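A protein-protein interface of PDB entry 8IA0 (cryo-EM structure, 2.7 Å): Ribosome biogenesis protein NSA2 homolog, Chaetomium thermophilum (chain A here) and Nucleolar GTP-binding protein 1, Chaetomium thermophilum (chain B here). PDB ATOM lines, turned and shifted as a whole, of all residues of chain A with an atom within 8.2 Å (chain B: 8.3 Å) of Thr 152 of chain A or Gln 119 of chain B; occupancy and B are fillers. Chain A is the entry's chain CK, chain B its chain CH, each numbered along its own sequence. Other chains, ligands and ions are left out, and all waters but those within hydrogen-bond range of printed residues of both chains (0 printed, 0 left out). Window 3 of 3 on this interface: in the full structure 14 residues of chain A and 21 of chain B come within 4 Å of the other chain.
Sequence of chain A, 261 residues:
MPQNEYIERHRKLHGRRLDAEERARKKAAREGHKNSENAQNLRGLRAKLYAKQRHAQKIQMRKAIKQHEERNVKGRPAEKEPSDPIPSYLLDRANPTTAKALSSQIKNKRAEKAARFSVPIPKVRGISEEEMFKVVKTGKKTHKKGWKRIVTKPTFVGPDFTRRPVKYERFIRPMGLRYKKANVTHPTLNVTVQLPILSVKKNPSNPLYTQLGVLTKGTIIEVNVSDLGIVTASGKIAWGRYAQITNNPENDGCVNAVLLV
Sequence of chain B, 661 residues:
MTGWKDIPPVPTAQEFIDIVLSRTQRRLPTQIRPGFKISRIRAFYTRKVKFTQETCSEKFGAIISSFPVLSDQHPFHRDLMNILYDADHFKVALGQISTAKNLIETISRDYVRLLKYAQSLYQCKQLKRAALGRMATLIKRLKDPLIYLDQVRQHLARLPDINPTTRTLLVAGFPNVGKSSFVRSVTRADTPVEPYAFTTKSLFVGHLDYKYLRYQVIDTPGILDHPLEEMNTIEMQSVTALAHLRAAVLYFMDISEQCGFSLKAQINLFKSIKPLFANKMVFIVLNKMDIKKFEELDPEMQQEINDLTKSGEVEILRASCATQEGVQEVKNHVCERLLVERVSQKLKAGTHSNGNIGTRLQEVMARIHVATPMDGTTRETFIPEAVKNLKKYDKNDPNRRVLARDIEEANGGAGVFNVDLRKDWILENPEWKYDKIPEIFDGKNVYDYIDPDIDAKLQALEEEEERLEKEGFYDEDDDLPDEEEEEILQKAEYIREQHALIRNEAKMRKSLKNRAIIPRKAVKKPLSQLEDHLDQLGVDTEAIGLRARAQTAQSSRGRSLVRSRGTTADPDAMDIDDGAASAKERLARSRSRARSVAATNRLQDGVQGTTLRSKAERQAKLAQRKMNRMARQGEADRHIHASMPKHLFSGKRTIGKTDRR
The side-chain amide nitrogen (NE2) of Gln 123 of chain B sits at hydrogen-bond distance from the backbone carbonyl oxygen (O) of Glu 250 of chain A (3.2 Å).
The backbone NH (N) of Thr 155 of chain A sits at hydrogen-bond distance from the backbone carbonyl oxygen (O) of Leu 177 of chain A, 3.0 Å away. The backbone NH (N) of Gln 119 of chain B lies within hydrogen-bond range of the side-chain amide oxygen (OE1) of Gln 123 of chain B (3.1 Å). The side-chain hydroxyl (OG) of Ser 120 of chain B lies within hydrogen-bond range of the backbone NH (N) of Gln 123 of chain B, at 3.4 Å. The backbone carbonyl oxygen of Tyr 117 of chain B lies close to the side-chain amide oxygen of Gln 119 of chain B (3.4 Å).
Among the printed residues, pairs that only touch across the chains: Thr 152 of chain A with Gln 119 of chain B, Pro 174 of chain A with Tyr 117 of chain B, Glu 250 of chain A with Leu 127 of chain B, Thr 152 of chain A with Tyr 117 of chain B and Leu 177 of chain A with Leu 114 of chain B.
Of chain B, only Tyr 117 and Gln 119 come within 4 Å of Thr 152 of chain A. Of chain A, only Thr 152 (3.3 Å) comes within 4 Å of Gln 119 of chain B. No residue of chain A comes within 4 Å of Ala 118 of chain B. No residue of chain A comes within 4 Å of Ser 120 of chain B. Of the printed residues of chain A, Gln 123 of chain B touches Glu 250 (3.2 Å). Of the printed residues of chain A, Leu 127 of chain B touches Glu 250. Printed residues of chain A within 4 Å of Tyr 117 of chain B: Thr 152 and Pro 174. Printed residues of chain B within 4 Å of Leu 177 of chain A: Leu 114 (3.7 Å). Thr 155 of chain A touches none of the printed residues of chain B. The nearest residue of chain B that does not touch Thr 152 of chain A is Gln 123 of chain B (5.0 Å). The nearest residue of chain A that does not touch Gln 119 of chain B is Ile 150 of chain A (6.5 Å). The nearest printed residue of chain A that does not touch Leu 114 of chain B is Pro 249 of chain A (5.5 Å).
Of the 15 printed residues of chain B, 5 touch a printed residue of chain A. Of the 15 printed residues of chain A, 4 touch a printed residue of chain B. Hydrophobic or aromatic side chains of chain A within 4 Å of the printed part of chain B: Pro 174 and Leu 177. Among the printed residues, 6 pairs touch across the chains. Among the printed residues, no Asp or Glu carboxylate lies within 4 Å of a Lys or Arg side-chain nitrogen of the other chain.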
ATOM      1  N   ARG A 149       4.657 -15.916  28.891  1.00  0.00           N
ATOM      2  CA  ARG A 149       4.520 -17.123  28.082  1.00  0.00           C
ATOM      3  C   ARG A 149       5.831 -17.891  28.178  1.00  0.00           C
ATOM      4  O   ARG A 149       6.778 -17.618  27.434  1.00  0.00           O
ATOM      5  CB  ARG A 149       4.175 -16.803  26.632  1.00  0.00           C
ATOM      6  CG  ARG A 149       2.868 -16.067  26.428  1.00  0.00           C
ATOM      7  CD  ARG A 149       2.851 -15.382  25.072  1.00  0.00           C
ATOM      8  NE  ARG A 149       1.531 -14.870  24.726  1.00  0.00           N
ATOM      9  CZ  ARG A 149       1.315 -13.835  23.926  1.00  0.00           C
ATOM     10  NH1 ARG A 149       2.316 -13.151  23.397  1.00  0.00           N
ATOM     11  NH2 ARG A 149       0.064 -13.480  23.649  1.00  0.00           N
ATOM     12  N   ILE A 150       5.885 -18.849  29.095  1.00  0.00           N
ATOM     13  CA  ILE A 150       7.064 -19.691  29.244  1.00  0.00           C
ATOM     14  C   ILE A 150       7.057 -20.722  28.124  1.00  0.00           C
ATOM     15  O   ILE A 150       6.128 -21.527  28.013  1.00  0.00           O
ATOM     16  CB  ILE A 150       7.095 -20.366  30.622  1.00  0.00           C
ATOM     17  CG1 ILE A 150       7.530 -19.365  31.693  1.00  0.00           C
ATOM     18  CG2 ILE A 150       8.028 -21.569  30.607  1.00  0.00           C
ATOM     19  CD1 ILE A 150       8.050 -20.005  32.964  1.00  0.00           C
ATOM     20  N   VAL A 151       8.087 -20.690  27.284  1.00  0.00           N
ATOM     21  CA  VAL A 151       8.236 -21.670  26.215  1.00  0.00           C
ATOM     22  C   VAL A 151       8.749 -22.959  26.845  1.00  0.00           C
ATOM     23  O   VAL A 151       9.901 -23.036  27.277  1.00  0.00           O
ATOM     24  CB  VAL A 151       9.181 -21.168  25.119  1.00  0.00           C
ATOM     25  CG1 VAL A 151       9.261 -22.177  23.987  1.00  0.00           C
ATOM     26  CG2 VAL A 151       8.723 -19.816  24.603  1.00  0.00           C
ATOM     27  N   THR A 152       7.892 -23.974  26.899  1.00  0.00           N
ATOM     28  CA  THR A 152       8.207 -25.228  27.567  1.00  0.00           C
ATOM     29  C   THR A 152       8.915 -26.221  26.656  1.00  0.00           C
ATOM     30  O   THR A 152       9.175 -27.352  27.077  1.00  0.00           O
ATOM     31  CB  THR A 152       6.930 -25.859  28.125  1.00  0.00           C
ATOM     32  OG1 THR A 152       5.842 -25.614  27.225  1.00  0.00           O
ATOM     33  CG2 THR A 152       6.597 -25.263  29.482  1.00  0.00           C
ATOM     34  N   LYS A 153       9.225 -25.834  25.450  1.00  0.00           N
ATOM     35  CA  LYS A 153       9.941 -26.665  24.501  1.00  0.00           C
ATOM     36  C   LYS A 153      11.438 -26.388  24.561  1.00  0.00           C
ATOM     37  O   LYS A 153      11.857 -25.284  24.919  1.00  0.00           O
ATOM     38  CB  LYS A 153       9.433 -26.414  23.079  1.00  0.00           C
ATOM     39  CG  LYS A 153       8.448 -27.452  22.575  1.00  0.00           C
ATOM     40  CD  LYS A 153       7.028 -27.122  22.979  1.00  0.00           C
ATOM     41  CE  LYS A 153       6.036 -27.909  22.143  1.00  0.00           C
ATOM     42  NZ  LYS A 153       6.464 -29.324  21.976  1.00  0.00           N
ATOM     43  N   PRO A 154      12.270 -27.378  24.237  1.00  0.00           N
ATOM     44  CA  PRO A 154      13.717 -27.137  24.193  1.00  0.00           C
ATOM     45  C   PRO A 154      14.080 -26.135  23.108  1.00  0.00           C
ATOM     46  O   PRO A 154      13.480 -26.114  22.031  1.00  0.00           O
ATOM     47  CB  PRO A 154      14.294 -28.524  23.894  1.00  0.00           C
ATOM     48  CG  PRO A 154      13.186 -29.262  23.242  1.00  0.00           C
ATOM     49  CD  PRO A 154      11.933 -28.768  23.893  1.00  0.00           C
ATOM     50  N   THR A 155      15.075 -25.296  23.401  1.00  0.00           N
ATOM     51  CA  THR A 155      15.447 -24.193  22.525  1.00  0.00           C
ATOM     52  C   THR A 155      16.959 -24.105  22.366  1.00  0.00           C
ATOM     53  O   THR A 155      17.727 -24.715  23.112  1.00  0.00           O
ATOM     54  CB  THR A 155      14.932 -22.840  23.047  1.00  0.00           C
ATOM     55  OG1 THR A 155      15.722 -22.424  24.167  1.00  0.00           O
ATOM     56  CG2 THR A 155      13.470 -22.918  23.456  1.00  0.00           C
ATOM     57  N   ILE A 172       9.387 -16.243  27.031  1.00  0.00           N
ATOM     58  CA  ILE A 172      10.536 -16.479  27.894  1.00  0.00           C
ATOM     59  C   ILE A 172      10.978 -17.925  27.749  1.00  0.00           C
ATOM     60  O   ILE A 172      10.167 -18.853  27.847  1.00  0.00           O
ATOM     61  CB  ILE A 172      10.201 -16.138  29.357  1.00  0.00           C
ATOM     62  CG1 ILE A 172       9.971 -14.633  29.512  1.00  0.00           C
ATOM     63  CG2 ILE A 172      11.309 -16.606  30.284  1.00  0.00           C
ATOM     64  CD1 ILE A 172      10.998 -13.780  28.805  1.00  0.00           C
ATOM     65  N   ARG A 173      12.272 -18.117  27.509  1.00  0.00           N
ATOM     66  CA  ARG A 173      12.856 -19.436  27.316  1.00  0.00           C
ATOM     67  C   ARG A 173      13.767 -19.761  28.492  1.00  0.00           C
ATOM     68  O   ARG A 173      14.826 -19.128  28.639  1.00  0.00           O
ATOM     69  CB  ARG A 173      13.630 -19.483  26.000  1.00  0.00           C
ATOM     70  CG  ARG A 173      12.763 -19.229  24.778  1.00  0.00           C
ATOM     71  CD  ARG A 173      13.594 -18.878  23.558  1.00  0.00           C
ATOM     72  NE  ARG A 173      14.315 -17.623  23.728  1.00  0.00           N
ATOM     73  CZ  ARG A 173      15.060 -17.054  22.792  1.00  0.00           C
ATOM     74  NH1 ARG A 173      15.205 -17.600  21.597  1.00  0.00           N
ATOM     75  NH2 ARG A 173      15.681 -15.911  23.063  1.00  0.00           N
ATOM     76  N   PRO A 174      13.407 -20.715  29.346  1.00  0.00           N
ATOM     77  CA  PRO A 174      14.209 -20.989  30.543  1.00  0.00           C
ATOM     78  C   PRO A 174      15.603 -21.516  30.234  1.00  0.00           C
ATOM     79  O   PRO A 174      15.850 -22.139  29.198  1.00  0.00           O
ATOM     80  CB  PRO A 174      13.381 -22.037  31.296  1.00  0.00           C
ATOM     81  CG  PRO A 174      12.383 -22.544  30.315  1.00  0.00           C
ATOM     82  CD  PRO A 174      12.130 -21.442  29.353  1.00  0.00           C
ATOM     83  N   LEU A 177      16.144 -25.406  29.694  1.00  0.00           N
ATOM     84  CA  LEU A 177      15.727 -25.988  28.428  1.00  0.00           C
ATOM     85  C   LEU A 177      16.641 -25.618  27.269  1.00  0.00           C
ATOM     86  O   LEU A 177      16.286 -25.881  26.117  1.00  0.00           O
ATOM     87  CB  LEU A 177      14.289 -25.570  28.102  1.00  0.00           C
ATOM     88  CG  LEU A 177      13.176 -26.347  28.810  1.00  0.00           C
ATOM     89  CD1 LEU A 177      11.839 -25.650  28.640  1.00  0.00           C
ATOM     90  CD2 LEU A 177      13.105 -27.772  28.288  1.00  0.00           C
ATOM     91  N   TYR A 209       8.168 -21.043  15.936  1.00  0.00           N
ATOM     92  CA  TYR A 209       9.140 -21.896  16.609  1.00  0.00           C
ATOM     93  C   TYR A 209      10.528 -21.742  16.002  1.00  0.00           C
ATOM     94  O   TYR A 209      11.535 -21.817  16.715  1.00  0.00           O
ATOM     95  CB  TYR A 209       8.685 -23.354  16.551  1.00  0.00           C
ATOM     96  CG  TYR A 209       7.691 -23.725  17.625  1.00  0.00           C
ATOM     97  CD1 TYR A 209       7.217 -22.775  18.517  1.00  0.00           C
ATOM     98  CD2 TYR A 209       7.224 -25.025  17.746  1.00  0.00           C
ATOM     99  CE1 TYR A 209       6.311 -23.110  19.500  1.00  0.00           C
ATOM    100  CE2 TYR A 209       6.317 -25.369  18.726  1.00  0.00           C
ATOM    101  CZ  TYR A 209       5.863 -24.407  19.599  1.00  0.00           C
ATOM    102  OH  TYR A 209       4.957 -24.746  20.578  1.00  0.00           O
ATOM    103  N   VAL A 214      13.044 -23.236  18.688  1.00  0.00           N
ATOM    104  CA  VAL A 214      12.528 -24.442  19.324  1.00  0.00           C
ATOM    105  C   VAL A 214      13.009 -25.667  18.561  1.00  0.00           C
ATOM    106  O   VAL A 214      12.835 -25.768  17.340  1.00  0.00           O
ATOM    107  CB  VAL A 214      10.996 -24.391  19.395  1.00  0.00           C
ATOM    108  CG1 VAL A 214      10.435 -25.760  19.713  1.00  0.00           C
ATOM    109  CG2 VAL A 214      10.549 -23.377  20.430  1.00  0.00           C
ATOM    110  N   PRO A 249      13.613 -34.029  21.675  1.00  0.00           N
ATOM    111  CA  PRO A 249      14.432 -33.487  22.771  1.00  0.00           C
ATOM    112  C   PRO A 249      13.644 -33.178  24.031  1.00  0.00           C
ATOM    113  O   PRO A 249      14.233 -33.082  25.114  1.00  0.00           O
ATOM    114  CB  PRO A 249      15.040 -32.220  22.154  1.00  0.00           C
ATOM    115  CG  PRO A 249      14.994 -32.449  20.686  1.00  0.00           C
ATOM    116  CD  PRO A 249      13.758 -33.250  20.435  1.00  0.00           C
ATOM    117  N   GLU A 250      12.326 -33.003  23.924  1.00  0.00           N
ATOM    118  CA  GLU A 250      11.526 -32.732  25.114  1.00  0.00           C
ATOM    119  C   GLU A 250      11.357 -33.987  25.962  1.00  0.00           C
ATOM    120  O   GLU A 250      11.345 -33.914  27.196  1.00  0.00           O
ATOM    121  CB  GLU A 250      10.161 -32.156  24.728  1.00  0.00           C
ATOM    122  CG  GLU A 250       9.427 -32.877  23.603  1.00  0.00           C
ATOM    123  CD  GLU A 250       9.973 -32.549  22.227  1.00  0.00           C
ATOM    124  OE1 GLU A 250      10.638 -31.501  22.083  1.00  0.00           O
ATOM    125  OE2 GLU A 250       9.739 -33.340  21.288  1.00  0.00           O
ATOM    126  N   ILE B  38      -0.444 -31.661  38.274  1.00  0.00           N
ATOM    127  CA  ILE B  38       0.808 -31.730  37.526  1.00  0.00           C
ATOM    128  C   ILE B  38       1.994 -31.555  38.468  1.00  0.00           C
ATOM    129  O   ILE B  38       3.048 -32.179  38.287  1.00  0.00           O
ATOM    130  CB  ILE B  38       0.804 -30.687  36.390  1.00  0.00           C
ATOM    131  CG1 ILE B  38       2.091 -30.752  35.566  1.00  0.00           C
ATOM    132  CG2 ILE B  38       0.575 -29.284  36.936  1.00  0.00           C
ATOM    133  CD1 ILE B  38       2.534 -32.155  35.206  1.00  0.00           C
ATOM    134  N   ILE B  41       2.663 -34.885  40.105  1.00  0.00           N
ATOM    135  CA  ILE B  41       3.344 -35.781  39.175  1.00  0.00           C
ATOM    136  C   ILE B  41       4.808 -35.387  39.027  1.00  0.00           C
ATOM    137  O   ILE B  41       5.697 -36.246  39.002  1.00  0.00           O
ATOM    138  CB  ILE B  41       2.617 -35.793  37.818  1.00  0.00           C
ATOM    139  CG1 ILE B  41       1.270 -36.500  37.945  1.00  0.00           C
ATOM    140  CG2 ILE B  41       3.467 -36.468  36.759  1.00  0.00           C
ATOM    141  CD1 ILE B  41       0.191 -35.906  37.074  1.00  0.00           C
ATOM    142  N   ARG B  42       5.083 -34.084  38.927  1.00  0.00           N
ATOM    143  CA  ARG B  42       6.465 -33.624  38.831  1.00  0.00           C
ATOM    144  C   ARG B  42       7.262 -34.011  40.070  1.00  0.00           C
ATOM    145  O   ARG B  42       8.413 -34.446  39.964  1.00  0.00           O
ATOM    146  CB  ARG B  42       6.510 -32.110  38.626  1.00  0.00           C
ATOM    147  CG  ARG B  42       6.185 -31.647  37.221  1.00  0.00           C
ATOM    148  CD  ARG B  42       5.923 -30.154  37.200  1.00  0.00           C
ATOM    149  NE  ARG B  42       5.259 -29.728  35.977  1.00  0.00           N
ATOM    150  CZ  ARG B  42       4.740 -28.523  35.790  1.00  0.00           C
ATOM    151  NH1 ARG B  42       4.790 -27.596  36.731  1.00  0.00           N
ATOM    152  NH2 ARG B  42       4.154 -28.241  34.630  1.00  0.00           N
ATOM    153  N   LEU B 114      14.705 -30.290  33.851  1.00  0.00           N
ATOM    154  CA  LEU B 114      13.762 -30.594  32.781  1.00  0.00           C
ATOM    155  C   LEU B 114      12.397 -30.981  33.336  1.00  0.00           C
ATOM    156  O   LEU B 114      11.362 -30.576  32.797  1.00  0.00           O
ATOM    157  CB  LEU B 114      14.314 -31.711  31.899  1.00  0.00           C
ATOM    158  CG  LEU B 114      15.535 -31.374  31.046  1.00  0.00           C
ATOM    159  CD1 LEU B 114      15.990 -32.590  30.261  1.00  0.00           C
ATOM    160  CD2 LEU B 114      15.230 -30.218  30.115  1.00  0.00           C
ATOM    161  N   LEU B 115      12.377 -31.769  34.414  1.00  0.00           N
ATOM    162  CA  LEU B 115      11.112 -32.227  34.979  1.00  0.00           C
ATOM    163  C   LEU B 115      10.282 -31.063  35.504  1.00  0.00           C
ATOM    164  O   LEU B 115       9.048 -31.102  35.458  1.00  0.00           O
ATOM    165  CB  LEU B 115      11.367 -33.242  36.092  1.00  0.00           C
ATOM    166  CG  LEU B 115      11.607 -34.693  35.682  1.00  0.00           C
ATOM    167  CD1 LEU B 115      12.149 -35.487  36.853  1.00  0.00           C
ATOM    168  CD2 LEU B 115      10.329 -35.320  35.160  1.00  0.00           C
ATOM    169  N   LYS B 116      10.941 -30.018  36.007  1.00  0.00           N
ATOM    170  CA  LYS B 116      10.214 -28.884  36.563  1.00  0.00           C
ATOM    171  C   LYS B 116       9.465 -28.093  35.498  1.00  0.00           C
ATOM    172  O   LYS B 116       8.607 -27.274  35.840  1.00  0.00           O
ATOM    173  CB  LYS B 116      11.175 -27.977  37.335  1.00  0.00           C
ATOM    174  CG  LYS B 116      11.636 -26.737  36.591  1.00  0.00           C
ATOM    175  CD  LYS B 116      12.597 -25.902  37.433  1.00  0.00           C
ATOM    176  CE  LYS B 116      12.125 -25.726  38.874  1.00  0.00           C
ATOM    177  NZ  LYS B 116      10.686 -25.350  38.989  1.00  0.00           N
ATOM    178  N   TYR B 117       9.760 -28.324  34.220  1.00  0.00           N
ATOM    179  CA  TYR B 117       9.032 -27.700  33.125  1.00  0.00           C
ATOM    180  C   TYR B 117       8.188 -28.692  32.337  1.00  0.00           C
ATOM    181  O   TYR B 117       7.597 -28.312  31.322  1.00  0.00           O
ATOM    182  CB  TYR B 117      10.008 -26.986  32.183  1.00  0.00           C
ATOM    183  CG  TYR B 117      10.731 -25.831  32.832  1.00  0.00           C
ATOM    184  CD1 TYR B 117      10.033 -24.741  33.332  1.00  0.00           C
ATOM    185  CD2 TYR B 117      12.111 -25.835  32.956  1.00  0.00           C
ATOM    186  CE1 TYR B 117      10.689 -23.690  33.931  1.00  0.00           C
ATOM    187  CE2 TYR B 117      12.776 -24.787  33.554  1.00  0.00           C
ATOM    188  CZ  TYR B 117      12.060 -23.717  34.041  1.00  0.00           C
ATOM    189  OH  TYR B 117      12.717 -22.668  34.637  1.00  0.00           O
ATOM    190  N   ALA B 118       8.117 -29.947  32.773  1.00  0.00           N
ATOM    191  CA  ALA B 118       7.337 -30.949  32.066  1.00  0.00           C
ATOM    192  C   ALA B 118       5.844 -30.654  32.190  1.00  0.00           C
ATOM    193  O   ALA B 118       5.379 -30.049  33.159  1.00  0.00           O
ATOM    194  CB  ALA B 118       7.651 -32.345  32.599  1.00  0.00           C
ATOM    195  N   GLN B 119       5.085 -31.104  31.189  1.00  0.00           N
ATOM    196  CA  GLN B 119       3.694 -30.701  31.051  1.00  0.00           C
ATOM    197  C   GLN B 119       2.683 -31.837  31.133  1.00  0.00           C
ATOM    198  O   GLN B 119       1.483 -31.564  31.027  1.00  0.00           O
ATOM    199  CB  GLN B 119       3.484 -29.959  29.722  1.00  0.00           C
ATOM    200  CG  GLN B 119       4.259 -28.656  29.612  1.00  0.00           C
ATOM    201  CD  GLN B 119       3.712 -27.574  30.516  1.00  0.00           C
ATOM    202  OE1 GLN B 119       4.443 -26.992  31.317  1.00  0.00           O
ATOM    203  NE2 GLN B 119       2.421 -27.298  30.395  1.00  0.00           N
ATOM    204  N   SER B 120       3.109 -33.083  31.322  1.00  0.00           N
ATOM    205  CA  SER B 120       2.177 -34.201  31.398  1.00  0.00           C
ATOM    206  C   SER B 120       2.889 -35.395  32.016  1.00  0.00           C
ATOM    207  O   SER B 120       4.111 -35.399  32.179  1.00  0.00           O
ATOM    208  CB  SER B 120       1.613 -34.555  30.020  1.00  0.00           C
ATOM    209  OG  SER B 120       2.565 -35.259  29.248  1.00  0.00           O
ATOM    210  N   LEU B 121       2.099 -36.413  32.364  1.00  0.00           N
ATOM    211  CA  LEU B 121       2.664 -37.618  32.962  1.00  0.00           C
ATOM    212  C   LEU B 121       3.566 -38.355  31.983  1.00  0.00           C
ATOM    213  O   LEU B 121       4.617 -38.878  32.372  1.00  0.00           O
ATOM    214  CB  LEU B 121       1.547 -38.536  33.457  1.00  0.00           C
ATOM    215  CG  LEU B 121       2.006 -39.716  34.315  1.00  0.00           C
ATOM    216  CD1 LEU B 121       1.107 -39.883  35.523  1.00  0.00           C
ATOM    217  CD2 LEU B 121       2.043 -40.997  33.500  1.00  0.00           C
ATOM    218  N   TYR B 122       3.169 -38.418  30.711  1.00  0.00           N
ATOM    219  CA  TYR B 122       3.981 -39.108  29.714  1.00  0.00           C
ATOM    220  C   TYR B 122       5.355 -38.463  29.584  1.00  0.00           C
ATOM    221  O   TYR B 122       6.376 -39.158  29.531  1.00  0.00           O
ATOM    222  CB  TYR B 122       3.261 -39.117  28.366  1.00  0.00           C
ATOM    223  CG  TYR B 122       4.075 -39.722  27.249  1.00  0.00           C
ATOM    224  CD1 TYR B 122       4.210 -41.095  27.129  1.00  0.00           C
ATOM    225  CD2 TYR B 122       4.714 -38.919  26.318  1.00  0.00           C
ATOM    226  CE1 TYR B 122       4.953 -41.653  26.112  1.00  0.00           C
ATOM    227  CE2 TYR B 122       5.462 -39.468  25.299  1.00  0.00           C
ATOM    228  CZ  TYR B 122       5.578 -40.834  25.200  1.00  0.00           C
ATOM    229  OH  TYR B 122       6.320 -41.386  24.184  1.00  0.00           O
ATOM    230  N   GLN B 123       5.401 -37.131  29.535  1.00  0.00           N
ATOM    231  CA  GLN B 123       6.683 -36.443  29.434  1.00  0.00           C
ATOM    232  C   GLN B 123       7.517 -36.632  30.694  1.00  0.00           C
ATOM    233  O   GLN B 123       8.738 -36.808  30.618  1.00  0.00           O
ATOM    234  CB  GLN B 123       6.464 -34.958  29.156  1.00  0.00           C
ATOM    235  CG  GLN B 123       7.522 -34.344  28.263  1.00  0.00           C
ATOM    236  CD  GLN B 123       7.570 -32.840  28.376  1.00  0.00           C
ATOM    237  OE1 GLN B 123       6.590 -32.204  28.762  1.00  0.00           O
ATOM    238  NE2 GLN B 123       8.715 -32.259  28.046  1.00  0.00           N
ATOM    239  N   CYS B 124       6.878 -36.590  31.864  1.00  0.00           N
ATOM    240  CA  CYS B 124       7.599 -36.834  33.108  1.00  0.00           C
ATOM    241  C   CYS B 124       8.164 -38.247  33.144  1.00  0.00           C
ATOM    242  O   CYS B 124       9.299 -38.461  33.588  1.00  0.00           O
ATOM    243  CB  CYS B 124       6.680 -36.601  34.306  1.00  0.00           C
ATOM    244  SG  CYS B 124       6.235 -34.883  34.621  1.00  0.00           S
ATOM    245  N   LEU B 127      11.272 -38.620  30.806  1.00  0.00           N
ATOM    246  CA  LEU B 127      12.469 -37.993  31.358  1.00  0.00           C
ATOM    247  C   LEU B 127      13.065 -38.834  32.476  1.00  0.00           C
ATOM    248  O   LEU B 127      14.291 -38.955  32.586  1.00  0.00           O
ATOM    249  CB  LEU B 127      12.139 -36.588  31.857  1.00  0.00           C
ATOM    250  CG  LEU B 127      11.913 -35.544  30.766  1.00  0.00           C
ATOM    251  CD1 LEU B 127      11.228 -34.314  31.327  1.00  0.00           C
ATOM    252  CD2 LEU B 127      13.228 -35.176  30.109  1.00  0.00           C
